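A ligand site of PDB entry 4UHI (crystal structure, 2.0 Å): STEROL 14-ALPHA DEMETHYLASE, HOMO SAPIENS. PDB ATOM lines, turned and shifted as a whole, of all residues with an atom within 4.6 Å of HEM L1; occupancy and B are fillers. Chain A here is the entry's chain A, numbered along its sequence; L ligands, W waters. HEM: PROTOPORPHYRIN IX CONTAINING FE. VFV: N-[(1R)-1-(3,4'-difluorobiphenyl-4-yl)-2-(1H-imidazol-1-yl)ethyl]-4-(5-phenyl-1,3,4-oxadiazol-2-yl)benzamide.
The backbone NH of Cys 389 lies within hydrogen-bond range of the backbone carbonyl oxygen of Phe 382.
The side-chain sulfur of Cys 389 lies close to the backbone NH of Gly 391 (3.2 Å).
The side-chain amino group (NZ) of Lys 96 sits at hydrogen-bond distance from the backbone carbonyl oxygen (O) of Arg 388 (2.9 Å).
The backbone carbonyl oxygen (O) of Arg 386 is in hydrogen-bond range of the side-chain amino group (NZ) of Lys 96 (3.0 Å).
The side-chain hydroxyl (OG1) of Thr 255 sits at hydrogen-bond distance from the backbone carbonyl oxygen (O) of Ala 251 (2.5 Å).
The side-chain hydroxyl of Thr 259 sits at hydrogen-bond distance from the backbone carbonyl oxygen of Thr 255 (2.8 Å).
Merely in contact with HEM L1: Tyr 71 (3.9 Å), Phe 92 (3.4 Å), Leu 103 (3.9 Å), Leu 248 (3.7 Å), Ala 251 (3.5 Å), Gly 252 (3.9 Å), Thr 255 (3.5 Å), Pro 316 (3.5 Å), Ile 317 (3.3 Å), Met 320 (3.5 Å), Pro 381 (3.3 Å), Phe 382 (3.3 Å), Gly 383 (3.6 Å), Arg 388 (3.8 Å), Ile 390 (3.5 Å), Gly 391 (3.6 Å), Phe 394 (3.8 Å) and Ala 395 (3.6 Å).
Hydrophobic or aromatic side chains that line HEM L1: Tyr 85, Phe 92, Leu 103, Leu 248, Ala 251, Pro 316, Ile 317, Met 320, Phe 382, His 387, Ile 390, Phe 394 and Ala 395.
Within 4 Å of HEM L1: Tyr 71, Tyr 85, Phe 92, Lys 96, Leu 103, Leu 248, Ala 251, Gly 252, Thr 255, Pro 316, Ile 317, Met 320, Arg 322, Pro 381, Phe 382, Gly 383, His 387, Arg 388, Cys 389, Ile 390, Gly 391, Phe 394 and Ala 395.
An iron atom (FE) of HEM L1 is bound by a nitrogen (NAX) of VFV L2 (2.0 Å).
The side-chain sulfur (SG) of Cys 389 is bound to an iron atom (FE) of HEM L1, at 2.3 Å.
An oxygen (O2D) of HEM L1 is in salt-bridge range of the side-chain amino group of Lys 96, at 2.7 Å.
NH2 of Arg 322 lies within salt-bridge range of O2A of HEM L1 (2.7 Å).
A ring nitrogen (ND1) of His 387 lies within hydrogen-bond range of an oxygen (O1D) of HEM L1 (2.8 Å).
The side-chain hydroxyl of Tyr 85 sits at hydrogen-bond distance from an oxygen (O1D) of HEM L1.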
ATOM      1  N   TYR A  71      -8.631  19.820  -7.551  1.00  0.00           N
ATOM      2  CA  TYR A  71      -7.339  19.164  -7.252  1.00  0.00           C
ATOM      3  C   TYR A  71      -6.095  20.054  -7.376  1.00  0.00           C
ATOM      4  O   TYR A  71      -5.083  19.805  -6.720  1.00  0.00           O
ATOM      5  CB  TYR A  71      -7.126  17.945  -8.164  1.00  0.00           C
ATOM      6  CG  TYR A  71      -8.133  16.823  -8.009  1.00  0.00           C
ATOM      7  CD1 TYR A  71      -8.846  16.641  -6.824  1.00  0.00           C
ATOM      8  CD2 TYR A  71      -8.357  15.917  -9.054  1.00  0.00           C
ATOM      9  CE1 TYR A  71      -9.765  15.603  -6.695  1.00  0.00           C
ATOM     10  CE2 TYR A  71      -9.271  14.885  -8.930  1.00  0.00           C
ATOM     11  CZ  TYR A  71      -9.966  14.723  -7.758  1.00  0.00           C
ATOM     12  OH  TYR A  71     -10.872  13.685  -7.634  1.00  0.00           O
ATOM     13  N   TYR A  85      -2.669  19.064 -13.284  1.00  0.00           N
ATOM     14  CA  TYR A  85      -3.803  19.979 -13.092  1.00  0.00           C
ATOM     15  C   TYR A  85      -3.393  21.435 -13.131  1.00  0.00           C
ATOM     16  O   TYR A  85      -4.221  22.302 -12.940  1.00  0.00           O
ATOM     17  CB  TYR A  85      -4.526  19.661 -11.789  1.00  0.00           C
ATOM     18  CG  TYR A  85      -4.948  18.221 -11.718  1.00  0.00           C
ATOM     19  CD1 TYR A  85      -5.941  17.725 -12.579  1.00  0.00           C
ATOM     20  CD2 TYR A  85      -4.332  17.329 -10.854  1.00  0.00           C
ATOM     21  CE1 TYR A  85      -6.314  16.399 -12.543  1.00  0.00           C
ATOM     22  CE2 TYR A  85      -4.712  15.997 -10.813  1.00  0.00           C
ATOM     23  CZ  TYR A  85      -5.715  15.533 -11.660  1.00  0.00           C
ATOM     24  OH  TYR A  85      -6.090  14.191 -11.628  1.00  0.00           O
ATOM     25  N   PHE A  92      -2.710  18.352 -20.601  1.00  0.00           N
ATOM     26  CA  PHE A  92      -2.541  17.206 -19.747  1.00  0.00           C
ATOM     27  C   PHE A  92      -2.844  15.917 -20.530  1.00  0.00           C
ATOM     28  O   PHE A  92      -2.189  14.903 -20.340  1.00  0.00           O
ATOM     29  CB  PHE A  92      -3.430  17.333 -18.507  1.00  0.00           C
ATOM     30  CG  PHE A  92      -3.204  16.256 -17.474  1.00  0.00           C
ATOM     31  CD1 PHE A  92      -2.009  15.562 -17.408  1.00  0.00           C
ATOM     32  CD2 PHE A  92      -4.180  15.987 -16.523  1.00  0.00           C
ATOM     33  CE1 PHE A  92      -1.810  14.594 -16.448  1.00  0.00           C
ATOM     34  CE2 PHE A  92      -3.982  15.032 -15.545  1.00  0.00           C
ATOM     35  CZ  PHE A  92      -2.799  14.325 -15.514  1.00  0.00           C
ATOM     36  N   LYS A  96      -0.437  12.824 -20.958  1.00  0.00           N
ATOM     37  CA  LYS A  96      -0.827  11.439 -20.650  1.00  0.00           C
ATOM     38  C   LYS A  96      -0.504  10.454 -21.782  1.00  0.00           C
ATOM     39  O   LYS A  96      -0.117   9.320 -21.523  1.00  0.00           O
ATOM     40  CB  LYS A  96      -2.314  11.358 -20.276  1.00  0.00           C
ATOM     41  CG  LYS A  96      -2.630  12.027 -18.936  1.00  0.00           C
ATOM     42  CD  LYS A  96      -4.131  12.085 -18.662  1.00  0.00           C
ATOM     43  CE  LYS A  96      -4.728  10.713 -18.430  1.00  0.00           C
ATOM     44  NZ  LYS A  96      -6.171  10.785 -18.036  1.00  0.00           N
ATOM     45  N   LEU A 103       4.781   3.395 -21.417  1.00  0.00           N
ATOM     46  CA  LEU A 103       4.315   2.210 -20.750  1.00  0.00           C
ATOM     47  C   LEU A 103       3.901   1.168 -21.803  1.00  0.00           C
ATOM     48  O   LEU A 103       2.716   0.974 -22.122  1.00  0.00           O
ATOM     49  CB  LEU A 103       3.168   2.572 -19.813  1.00  0.00           C
ATOM     50  CG  LEU A 103       3.549   3.607 -18.746  1.00  0.00           C
ATOM     51  CD1 LEU A 103       2.315   4.151 -18.032  1.00  0.00           C
ATOM     52  CD2 LEU A 103       4.533   3.027 -17.730  1.00  0.00           C
ATOM     53  N   LEU A 150      10.221   3.351 -13.664  1.00  0.00           N
ATOM     54  CA  LEU A 150       9.640   4.566 -14.218  1.00  0.00           C
ATOM     55  C   LEU A 150      10.655   5.712 -14.373  1.00  0.00           C
ATOM     56  O   LEU A 150      10.468   6.584 -15.214  1.00  0.00           O
ATOM     57  CB  LEU A 150       8.460   5.031 -13.373  1.00  0.00           C
ATOM     58  CG  LEU A 150       7.317   4.025 -13.155  1.00  0.00           C
ATOM     59  CD1 LEU A 150       6.210   4.629 -12.294  1.00  0.00           C
ATOM     60  CD2 LEU A 150       6.747   3.553 -14.497  1.00  0.00           C
ATOM     61  N   LEU A 248       4.813  10.215 -11.897  1.00  0.00           N
ATOM     62  CA  LEU A 248       4.970   8.785 -12.101  1.00  0.00           C
ATOM     63  C   LEU A 248       5.248   8.068 -10.788  1.00  0.00           C
ATOM     64  O   LEU A 248       4.599   7.068 -10.490  1.00  0.00           O
ATOM     65  CB  LEU A 248       6.079   8.488 -13.103  1.00  0.00           C
ATOM     66  CG  LEU A 248       5.734   8.734 -14.563  1.00  0.00           C
ATOM     67  CD1 LEU A 248       6.998   8.737 -15.445  1.00  0.00           C
ATOM     68  CD2 LEU A 248       4.746   7.689 -15.033  1.00  0.00           C
ATOM     69  N   ALA A 251       2.169   8.196  -8.296  1.00  0.00           N
ATOM     70  CA  ALA A 251       1.088   7.319  -8.815  1.00  0.00           C
ATOM     71  C   ALA A 251       1.478   5.852  -8.719  1.00  0.00           C
ATOM     72  O   ALA A 251       0.659   4.992  -8.410  1.00  0.00           O
ATOM     73  CB  ALA A 251       0.799   7.672 -10.265  1.00  0.00           C
ATOM     74  N   GLY A 252       2.745   5.565  -8.999  1.00  0.00           N
ATOM     75  CA  GLY A 252       3.231   4.192  -8.993  1.00  0.00           C
ATOM     76  C   GLY A 252       3.406   3.538  -7.632  1.00  0.00           C
ATOM     77  O   GLY A 252       3.464   2.316  -7.539  1.00  0.00           O
ATOM     78  N   THR A 255      -0.655   3.435  -4.546  1.00  0.00           N
ATOM     79  CA  THR A 255      -1.756   2.660  -5.160  1.00  0.00           C
ATOM     80  C   THR A 255      -1.414   1.159  -5.203  1.00  0.00           C
ATOM     81  O   THR A 255      -2.245   0.328  -4.822  1.00  0.00           O
ATOM     82  CB  THR A 255      -2.104   3.169  -6.566  1.00  0.00           C
ATOM     83  OG1 THR A 255      -0.906   3.303  -7.336  1.00  0.00           O
ATOM     84  CG2 THR A 255      -2.807   4.521  -6.488  1.00  0.00           C
ATOM     85  N   SER A 256      -0.192   0.828  -5.608  1.00  0.00           N
ATOM     86  CA  SER A 256       0.244  -0.584  -5.638  1.00  0.00           C
ATOM     87  C   SER A 256       0.523  -1.169  -4.237  1.00  0.00           C
ATOM     88  O   SER A 256       0.207  -2.336  -3.975  1.00  0.00           O
ATOM     89  CB  SER A 256       1.479  -0.747  -6.518  1.00  0.00           C
ATOM     90  OG  SER A 256       1.121  -0.773  -7.890  1.00  0.00           O
ATOM     91  N   THR A 259      -2.746  -1.873  -2.225  1.00  0.00           N
ATOM     92  CA  THR A 259      -3.466  -2.972  -2.871  1.00  0.00           C
ATOM     93  C   THR A 259      -2.723  -4.278  -2.645  1.00  0.00           C
ATOM     94  O   THR A 259      -3.338  -5.315  -2.334  1.00  0.00           O
ATOM     95  CB  THR A 259      -3.682  -2.715  -4.370  1.00  0.00           C
ATOM     96  OG1 THR A 259      -4.403  -1.491  -4.554  1.00  0.00           O
ATOM     97  CG2 THR A 259      -4.466  -3.841  -5.006  1.00  0.00           C
ATOM     98  N   LEU A 311      -8.840  -4.978  -5.847  1.00  0.00           N
ATOM     99  CA  LEU A 311      -9.202  -3.643  -6.308  1.00  0.00           C
ATOM    100  C   LEU A 311     -10.706  -3.388  -6.191  1.00  0.00           C
ATOM    101  O   LEU A 311     -11.150  -2.259  -6.037  1.00  0.00           O
ATOM    102  CB  LEU A 311      -8.736  -3.411  -7.725  1.00  0.00           C
ATOM    103  CG  LEU A 311      -7.225  -3.317  -7.822  1.00  0.00           C
ATOM    104  CD1 LEU A 311      -6.800  -3.398  -9.272  1.00  0.00           C
ATOM    105  CD2 LEU A 311      -6.733  -2.023  -7.163  1.00  0.00           C
ATOM    106  N   PRO A 316      -7.725   1.755  -4.191  1.00  0.00           N
ATOM    107  CA  PRO A 316      -6.932   2.691  -3.402  1.00  0.00           C
ATOM    108  C   PRO A 316      -7.328   4.129  -3.664  1.00  0.00           C
ATOM    109  O   PRO A 316      -7.180   4.973  -2.794  1.00  0.00           O
ATOM    110  CB  PRO A 316      -5.504   2.441  -3.885  1.00  0.00           C
ATOM    111  CG  PRO A 316      -5.672   1.895  -5.254  1.00  0.00           C
ATOM    112  CD  PRO A 316      -6.913   1.070  -5.209  1.00  0.00           C
ATOM    113  N   ILE A 317      -7.834   4.394  -4.861  1.00  0.00           N
ATOM    114  CA  ILE A 317      -8.430   5.687  -5.136  1.00  0.00           C
ATOM    115  C   ILE A 317      -9.936   5.564  -4.964  1.00  0.00           C
ATOM    116  O   ILE A 317     -10.648   5.127  -5.877  1.00  0.00           O
ATOM    117  CB  ILE A 317      -7.988   6.217  -6.492  1.00  0.00           C
ATOM    118  CG1 ILE A 317      -6.465   6.366  -6.467  1.00  0.00           C
ATOM    119  CG2 ILE A 317      -8.633   7.560  -6.778  1.00  0.00           C
ATOM    120  CD1 ILE A 317      -5.838   6.741  -7.768  1.00  0.00           C
ATOM    121  N   MET A 320     -13.546   9.943  -6.826  1.00  0.00           N
ATOM    122  CA  MET A 320     -13.226  10.864  -7.886  1.00  0.00           C
ATOM    123  C   MET A 320     -14.198  12.037  -7.762  1.00  0.00           C
ATOM    124  O   MET A 320     -15.370  11.859  -7.432  1.00  0.00           O
ATOM    125  CB  MET A 320     -13.344  10.177  -9.245  1.00  0.00           C
ATOM    126  CG  MET A 320     -12.327   9.042  -9.409  1.00  0.00           C
ATOM    127  SD  MET A 320     -12.924   7.707 -10.451  1.00  0.00           S
ATOM    128  CE  MET A 320     -14.221   7.107  -9.372  1.00  0.00           C
ATOM    129  N   ARG A 322     -15.215  16.277  -9.039  1.00  0.00           N
ATOM    130  CA  ARG A 322     -15.133  17.305 -10.052  1.00  0.00           C
ATOM    131  C   ARG A 322     -15.929  18.509  -9.577  1.00  0.00           C
ATOM    132  O   ARG A 322     -16.870  18.361  -8.803  1.00  0.00           O
ATOM    133  CB  ARG A 322     -15.760  16.800 -11.362  1.00  0.00           C
ATOM    134  CG  ARG A 322     -15.202  15.485 -11.893  1.00  0.00           C
ATOM    135  CD  ARG A 322     -13.871  15.630 -12.603  1.00  0.00           C
ATOM    136  NE  ARG A 322     -13.487  14.365 -13.223  1.00  0.00           N
ATOM    137  CZ  ARG A 322     -12.719  13.416 -12.671  1.00  0.00           C
ATOM    138  NH1 ARG A 322     -12.141  13.574 -11.479  1.00  0.00           N
ATOM    139  NH2 ARG A 322     -12.489  12.295 -13.344  1.00  0.00           N
ATOM    140  N   VAL A 380     -14.851   0.227 -11.483  1.00  0.00           N
ATOM    141  CA  VAL A 380     -14.101   1.379 -12.026  1.00  0.00           C
ATOM    142  C   VAL A 380     -12.893   1.771 -11.171  1.00  0.00           C
ATOM    143  O   VAL A 380     -12.659   2.975 -10.926  1.00  0.00           O
ATOM    144  CB  VAL A 380     -15.031   2.612 -12.228  1.00  0.00           C
ATOM    145  CG1 VAL A 380     -16.039   2.347 -13.321  1.00  0.00           C
ATOM    146  CG2 VAL A 380     -15.761   2.944 -10.938  1.00  0.00           C
ATOM    147  N   PRO A 381     -12.096   0.784 -10.728  1.00  0.00           N
ATOM    148  CA  PRO A 381     -10.928   1.057  -9.884  1.00  0.00           C
ATOM    149  C   PRO A 381      -9.899   1.957 -10.550  1.00  0.00           C
ATOM    150  O   PRO A 381      -9.137   2.651  -9.855  1.00  0.00           O
ATOM    151  CB  PRO A 381     -10.325  -0.345  -9.653  1.00  0.00           C
ATOM    152  CG  PRO A 381     -10.757  -1.117 -10.838  1.00  0.00           C
ATOM    153  CD  PRO A 381     -12.180  -0.638 -11.084  1.00  0.00           C
ATOM    154  N   PHE A 382      -9.890   1.962 -11.883  1.00  0.00           N
ATOM    155  CA  PHE A 382      -9.001   2.844 -12.650  1.00  0.00           C
ATOM    156  C   PHE A 382      -9.741   3.981 -13.377  1.00  0.00           C
ATOM    157  O   PHE A 382      -9.160   4.660 -14.231  1.00  0.00           O
ATOM    158  CB  PHE A 382      -8.189   2.008 -13.649  1.00  0.00           C
ATOM    159  CG  PHE A 382      -7.280   1.003 -13.016  1.00  0.00           C
ATOM    160  CD1 PHE A 382      -6.019   1.381 -12.565  1.00  0.00           C
ATOM    161  CD2 PHE A 382      -7.675  -0.322 -12.849  1.00  0.00           C
ATOM    162  CE1 PHE A 382      -5.175   0.470 -11.987  1.00  0.00           C
ATOM    163  CE2 PHE A 382      -6.837  -1.239 -12.267  1.00  0.00           C
ATOM    164  CZ  PHE A 382      -5.575  -0.844 -11.834  1.00  0.00           C
ATOM    165  N   GLY A 383     -10.997   4.215 -13.004  1.00  0.00           N
ATOM    166  CA  GLY A 383     -11.781   5.283 -13.603  1.00  0.00           C
ATOM    167  C   GLY A 383     -12.219   4.962 -15.033  1.00  0.00           C
ATOM    168  O   GLY A 383     -12.248   3.797 -15.443  1.00  0.00           O
ATOM    169  N   ARG A 386     -12.156  10.855 -19.734  1.00  0.00           N
ATOM    170  CA  ARG A 386     -10.976  11.653 -20.060  1.00  0.00           C
ATOM    171  C   ARG A 386      -9.884  11.667 -18.965  1.00  0.00           C
ATOM    172  O   ARG A 386      -8.708  11.878 -19.264  1.00  0.00           O
ATOM    173  CB  ARG A 386     -11.390  13.089 -20.393  1.00  0.00           C
ATOM    174  CG  ARG A 386     -12.259  13.224 -21.641  1.00  0.00           C
ATOM    175  CD  ARG A 386     -12.865  14.616 -21.734  1.00  0.00           C
ATOM    176  NE  ARG A 386     -13.566  14.833 -22.991  1.00  0.00           N
ATOM    177  CZ  ARG A 386     -14.782  14.378 -23.275  1.00  0.00           C
ATOM    178  NH1 ARG A 386     -15.440  13.642 -22.384  1.00  0.00           N
ATOM    179  NH2 ARG A 386     -15.327  14.630 -24.454  1.00  0.00           N
ATOM    180  N   HIS A 387     -10.290  11.478 -17.696  1.00  0.00           N
ATOM    181  CA  HIS A 387      -9.332  11.463 -16.577  1.00  0.00           C
ATOM    182  C   HIS A 387      -8.936  10.048 -16.168  1.00  0.00           C
ATOM    183  O   HIS A 387      -8.342   9.856 -15.127  1.00  0.00           O
ATOM    184  CB  HIS A 387      -9.922  12.176 -15.357  1.00  0.00           C
ATOM    185  CG  HIS A 387     -10.176  13.636 -15.576  1.00  0.00           C
ATOM    186  ND1 HIS A 387      -9.187  14.592 -15.465  1.00  0.00           N
ATOM    187  CD2 HIS A 387     -11.309  14.306 -15.912  1.00  0.00           C
ATOM    188  CE1 HIS A 387      -9.698  15.784 -15.734  1.00  0.00           C
ATOM    189  NE2 HIS A 387     -10.980  15.630 -16.010  1.00  0.00           N
ATOM    190  N   ARG A 388      -9.272   9.054 -16.997  1.00  0.00           N
ATOM    191  CA  ARG A 388      -9.012   7.655 -16.634  1.00  0.00           C
ATOM    192  C   ARG A 388      -7.509   7.388 -16.502  1.00  0.00           C
ATOM    193  O   ARG A 388      -6.674   8.125 -17.020  1.00  0.00           O
ATOM    194  CB  ARG A 388      -9.627   6.703 -17.659  1.00  0.00           C
ATOM    195  CG  ARG A 388      -8.826   6.614 -18.960  1.00  0.00           C
ATOM    196  CD  ARG A 388      -9.322   5.505 -19.861  1.00  0.00           C
ATOM    197  NE  ARG A 388      -8.862   5.713 -21.233  1.00  0.00           N
ATOM    198  CZ  ARG A 388      -9.237   4.954 -22.277  1.00  0.00           C
ATOM    199  NH1 ARG A 388     -10.088   3.944 -22.104  1.00  0.00           N
ATOM    200  NH2 ARG A 388      -8.758   5.221 -23.487  1.00  0.00           N
ATOM    201  N   CYS A 389      -7.178   6.308 -15.806  1.00  0.00           N
ATOM    202  CA  CYS A 389      -5.804   5.981 -15.507  1.00  0.00           C
ATOM    203  C   CYS A 389      -5.031   5.500 -16.739  1.00  0.00           C
ATOM    204  O   CYS A 389      -5.589   4.798 -17.581  1.00  0.00           O
ATOM    205  CB  CYS A 389      -5.759   4.898 -14.453  1.00  0.00           C
ATOM    206  SG  CYS A 389      -4.121   4.608 -13.768  1.00  0.00           S
ATOM    207  N   ILE A 390      -3.756   5.856 -16.821  1.00  0.00           N
ATOM    208  CA  ILE A 390      -2.871   5.357 -17.864  1.00  0.00           C
ATOM    209  C   ILE A 390      -1.964   4.222 -17.386  1.00  0.00           C
ATOM    210  O   ILE A 390      -1.242   3.635 -18.172  1.00  0.00           O
ATOM    211  CB  ILE A 390      -2.054   6.497 -18.516  1.00  0.00           C
ATOM    212  CG1 ILE A 390      -1.426   7.419 -17.474  1.00  0.00           C
ATOM    213  CG2 ILE A 390      -2.940   7.344 -19.403  1.00  0.00           C
ATOM    214  CD1 ILE A 390       0.014   7.105 -17.157  1.00  0.00           C
ATOM    215  N   GLY A 391      -2.039   3.891 -16.094  1.00  0.00           N
ATOM    216  CA  GLY A 391      -1.011   3.062 -15.464  1.00  0.00           C
ATOM    217  C   GLY A 391      -1.483   1.672 -15.069  1.00  0.00           C
ATOM    218  O   GLY A 391      -0.757   0.940 -14.378  1.00  0.00           O
ATOM    219  N   PHE A 394       0.944  -1.194 -16.119  1.00  0.00           N
ATOM    220  CA  PHE A 394       2.122  -1.179 -15.268  1.00  0.00           C
ATOM    221  C   PHE A 394       1.841  -1.668 -13.859  1.00  0.00           C
ATOM    222  O   PHE A 394       2.596  -2.467 -13.300  1.00  0.00           O
ATOM    223  CB  PHE A 394       2.759   0.210 -15.173  1.00  0.00           C
ATOM    224  CG  PHE A 394       3.952   0.254 -14.258  1.00  0.00           C
ATOM    225  CD1 PHE A 394       5.186  -0.243 -14.676  1.00  0.00           C
ATOM    226  CD2 PHE A 394       3.829   0.720 -12.949  1.00  0.00           C
ATOM    227  CE1 PHE A 394       6.267  -0.260 -13.824  1.00  0.00           C
ATOM    228  CE2 PHE A 394       4.914   0.706 -12.087  1.00  0.00           C
ATOM    229  CZ  PHE A 394       6.139   0.216 -12.527  1.00  0.00           C
ATOM    230  N   ALA A 395       0.735  -1.214 -13.293  1.00  0.00           N
ATOM    231  CA  ALA A 395       0.387  -1.582 -11.926  1.00  0.00           C
ATOM    232  C   ALA A 395       0.209  -3.097 -11.825  1.00  0.00           C
ATOM    233  O   ALA A 395       0.633  -3.727 -10.862  1.00  0.00           O
ATOM    234  CB  ALA A 395      -0.867  -0.856 -11.458  1.00  0.00           C
HETATM  235  CHA HEM L   1      -5.952   8.343 -13.086  1.00  0.00           C
HETATM  236  CHB HEM L   1      -6.393   4.556 -10.203  1.00  0.00           C
HETATM  237  CHC HEM L   1      -1.744   3.362 -10.957  1.00  0.00           C
HETATM  238  CHD HEM L   1      -1.205   7.408 -13.496  1.00  0.00           C
HETATM  239  C1A HEM L   1      -6.451   7.385 -12.297  1.00  0.00           C
HETATM  240  C2A HEM L   1      -7.800   7.366 -11.848  1.00  0.00           C
HETATM  241  C3A HEM L   1      -7.921   6.302 -11.033  1.00  0.00           C
HETATM  242  C4A HEM L   1      -6.652   5.673 -10.948  1.00  0.00           C
HETATM  243  CMA HEM L   1      -9.196   5.877 -10.357  1.00  0.00           C
HETATM  244  CAA HEM L   1      -8.919   8.336 -12.228  1.00  0.00           C
HETATM  245  CBA HEM L   1      -8.869   9.594 -11.356  1.00  0.00           C
HETATM  246  CGA HEM L   1     -10.069  10.498 -11.583  1.00  0.00           C
HETATM  247  O1A HEM L   1     -10.287  11.480 -10.833  1.00  0.00           O
HETATM  248  O2A HEM L   1     -10.867  10.266 -12.504  1.00  0.00           O
HETATM  249  C1B HEM L   1      -5.143   3.909 -10.195  1.00  0.00           C
HETATM  250  C2B HEM L   1      -4.929   2.699  -9.491  1.00  0.00           C
HETATM  251  C3B HEM L   1      -3.628   2.327  -9.697  1.00  0.00           C
HETATM  252  C4B HEM L   1      -3.060   3.380 -10.544  1.00  0.00           C
HETATM  253  CMB HEM L   1      -5.966   1.950  -8.697  1.00  0.00           C
HETATM  254  CAB HEM L   1      -2.892   1.123  -9.235  1.00  0.00           C
HETATM  255  CBB HEM L   1      -3.484   0.071  -8.670  1.00  0.00           C
HETATM  256  C1C HEM L   1      -1.188   4.353 -11.733  1.00  0.00           C
HETATM  257  C2C HEM L   1       0.081   4.318 -12.257  1.00  0.00           C
HETATM  258  C3C HEM L   1       0.251   5.477 -13.000  1.00  0.00           C
HETATM  259  C4C HEM L   1      -0.959   6.207 -12.896  1.00  0.00           C
HETATM  260  CMC HEM L   1       1.049   3.171 -12.031  1.00  0.00           C
HETATM  261  CAC HEM L   1       1.404   5.892 -13.809  1.00  0.00           C
HETATM  262  CBC HEM L   1       2.323   5.016 -14.206  1.00  0.00           C
HETATM  263  C1D HEM L   1      -2.491   7.956 -13.546  1.00  0.00           C
HETATM  264  C2D HEM L   1      -2.782   9.174 -14.315  1.00  0.00           C
HETATM  265  C3D HEM L   1      -4.083   9.445 -14.197  1.00  0.00           C
HETATM  266  C4D HEM L   1      -4.621   8.366 -13.374  1.00  0.00           C
HETATM  267  CMD HEM L   1      -1.805  10.020 -15.089  1.00  0.00           C
HETATM  268  CAD HEM L   1      -4.832  10.583 -14.865  1.00  0.00           C
HETATM  269  CBD HEM L   1      -5.486  11.597 -13.928  1.00  0.00           C
HETATM  270  CGD HEM L   1      -6.309  12.585 -14.742  1.00  0.00           C
HETATM  271  O1D HEM L   1      -7.007  13.460 -14.164  1.00  0.00           O
HETATM  272  O2D HEM L   1      -6.299  12.559 -15.986  1.00  0.00           O
HETATM  273  NA  HEM L   1      -5.756   6.339 -11.719  1.00  0.00           N
HETATM  274  NB  HEM L   1      -4.027   4.260 -10.811  1.00  0.00           N
HETATM  275  NC  HEM L   1      -1.811   5.472 -12.149  1.00  0.00           N
HETATM  276  ND  HEM L   1      -3.623   7.487 -13.017  1.00  0.00           N
HETATM  277 FE   HEM L   1      -3.813   5.977 -11.932  1.00  0.00          FE
HETATM  278  CAO VFV L   2      -0.308  13.063 -13.251  1.00  0.00           C
HETATM  279  CAK VFV L   2       0.517  13.337 -14.352  1.00  0.00           C
HETATM  280  CBD VFV L   2       1.816  12.851 -14.394  1.00  0.00           C
HETATM  281  FAB VFV L   2       2.581  13.099 -15.410  1.00  0.00           F
HETATM  282  CAJ VFV L   2       2.292  12.096 -13.350  1.00  0.00           C
HETATM  283  CAN VFV L   2       1.477  11.820 -12.263  1.00  0.00           C
HETATM  284  CBG VFV L   2       0.187  12.315 -12.194  1.00  0.00           C
HETATM  285  CBJ VFV L   2      -0.610  11.998 -11.099  1.00  0.00           C
HETATM  286  CAV VFV L   2      -0.064  11.289 -10.028  1.00  0.00           C
HETATM  287  CBE VFV L   2      -0.862  10.943  -8.956  1.00  0.00           C
HETATM  288  FAC VFV L   2      -0.329  10.330  -8.026  1.00  0.00           F
HETATM  289  CAR VFV L   2      -1.966  12.331 -11.072  1.00  0.00           C
HETATM  290  CAS VFV L   2      -2.764  11.985 -10.000  1.00  0.00           C
HETATM  291  CBK VFV L   2      -2.222  11.316  -8.919  1.00  0.00           C
HETATM  292  CBN VFV L   2      -3.053  10.933  -7.834  1.00  0.00           C
HETATM  293  CAW VFV L   2      -4.163  10.022  -8.331  1.00  0.00           C
HETATM  294  NBO VFV L   2      -3.634   8.813  -8.944  1.00  0.00           N
HETATM  295  CAT VFV L   2      -2.658   8.025  -8.522  1.00  0.00           C
HETATM  296  CAG VFV L   2      -2.559   7.007  -9.396  1.00  0.00           C
HETATM  297  NAX VFV L   2      -3.464   7.208 -10.342  1.00  0.00           N
HETATM  298  CAU VFV L   2      -4.144   8.309 -10.050  1.00  0.00           C
HETATM  299  NBA VFV L   2      -3.744  12.035  -7.149  1.00  0.00           N
HETATM  300  CBC VFV L   2      -3.219  12.677  -6.085  1.00  0.00           C
HETATM  301  OAA VFV L   2      -2.134  12.350  -5.583  1.00  0.00           O
HETATM  302  CBF VFV L   2      -4.123  13.513  -5.388  1.00  0.00           C
HETATM  303  CAM VFV L   2      -3.958  13.562  -3.990  1.00  0.00           C
HETATM  304  CAQ VFV L   2      -4.835  14.289  -3.198  1.00  0.00           C
HETATM  305  CAL VFV L   2      -5.221  14.171  -5.967  1.00  0.00           C
HETATM  306  CAP VFV L   2      -6.100  14.911  -5.157  1.00  0.00           C
HETATM  307  CBI VFV L   2      -5.904  14.981  -3.776  1.00  0.00           C
HETATM  308  CBM VFV L   2      -6.746  15.627  -2.969  1.00  0.00           C
HETATM  309  OBB VFV L   2      -6.831  15.360  -1.685  1.00  0.00           O
HETATM  310  NAZ VFV L   2      -7.656  16.530  -3.309  1.00  0.00           N
HETATM  311  NAY VFV L   2      -8.255  16.836  -2.244  1.00  0.00           N
HETATM  312  CBL VFV L   2      -7.723  16.115  -1.254  1.00  0.00           C
HETATM  313  CBH VFV L   2      -8.108  16.143   0.033  1.00  0.00           C
HETATM  314  CAI VFV L   2      -7.248  15.710   1.042  1.00  0.00           C
HETATM  315  CAF VFV L   2      -7.674  15.720   2.383  1.00  0.00           C
HETATM  316  CAD VFV L   2      -8.961  16.163   2.693  1.00  0.00           C
HETATM  317  CAE VFV L   2      -9.818  16.599   1.671  1.00  0.00           C
HETATM  318  CAH VFV L   2      -9.392  16.589   0.352  1.00  0.00           C
HETATM  319  O   HOH W   1     -11.746   8.449 -14.496  1.00  0.00           O
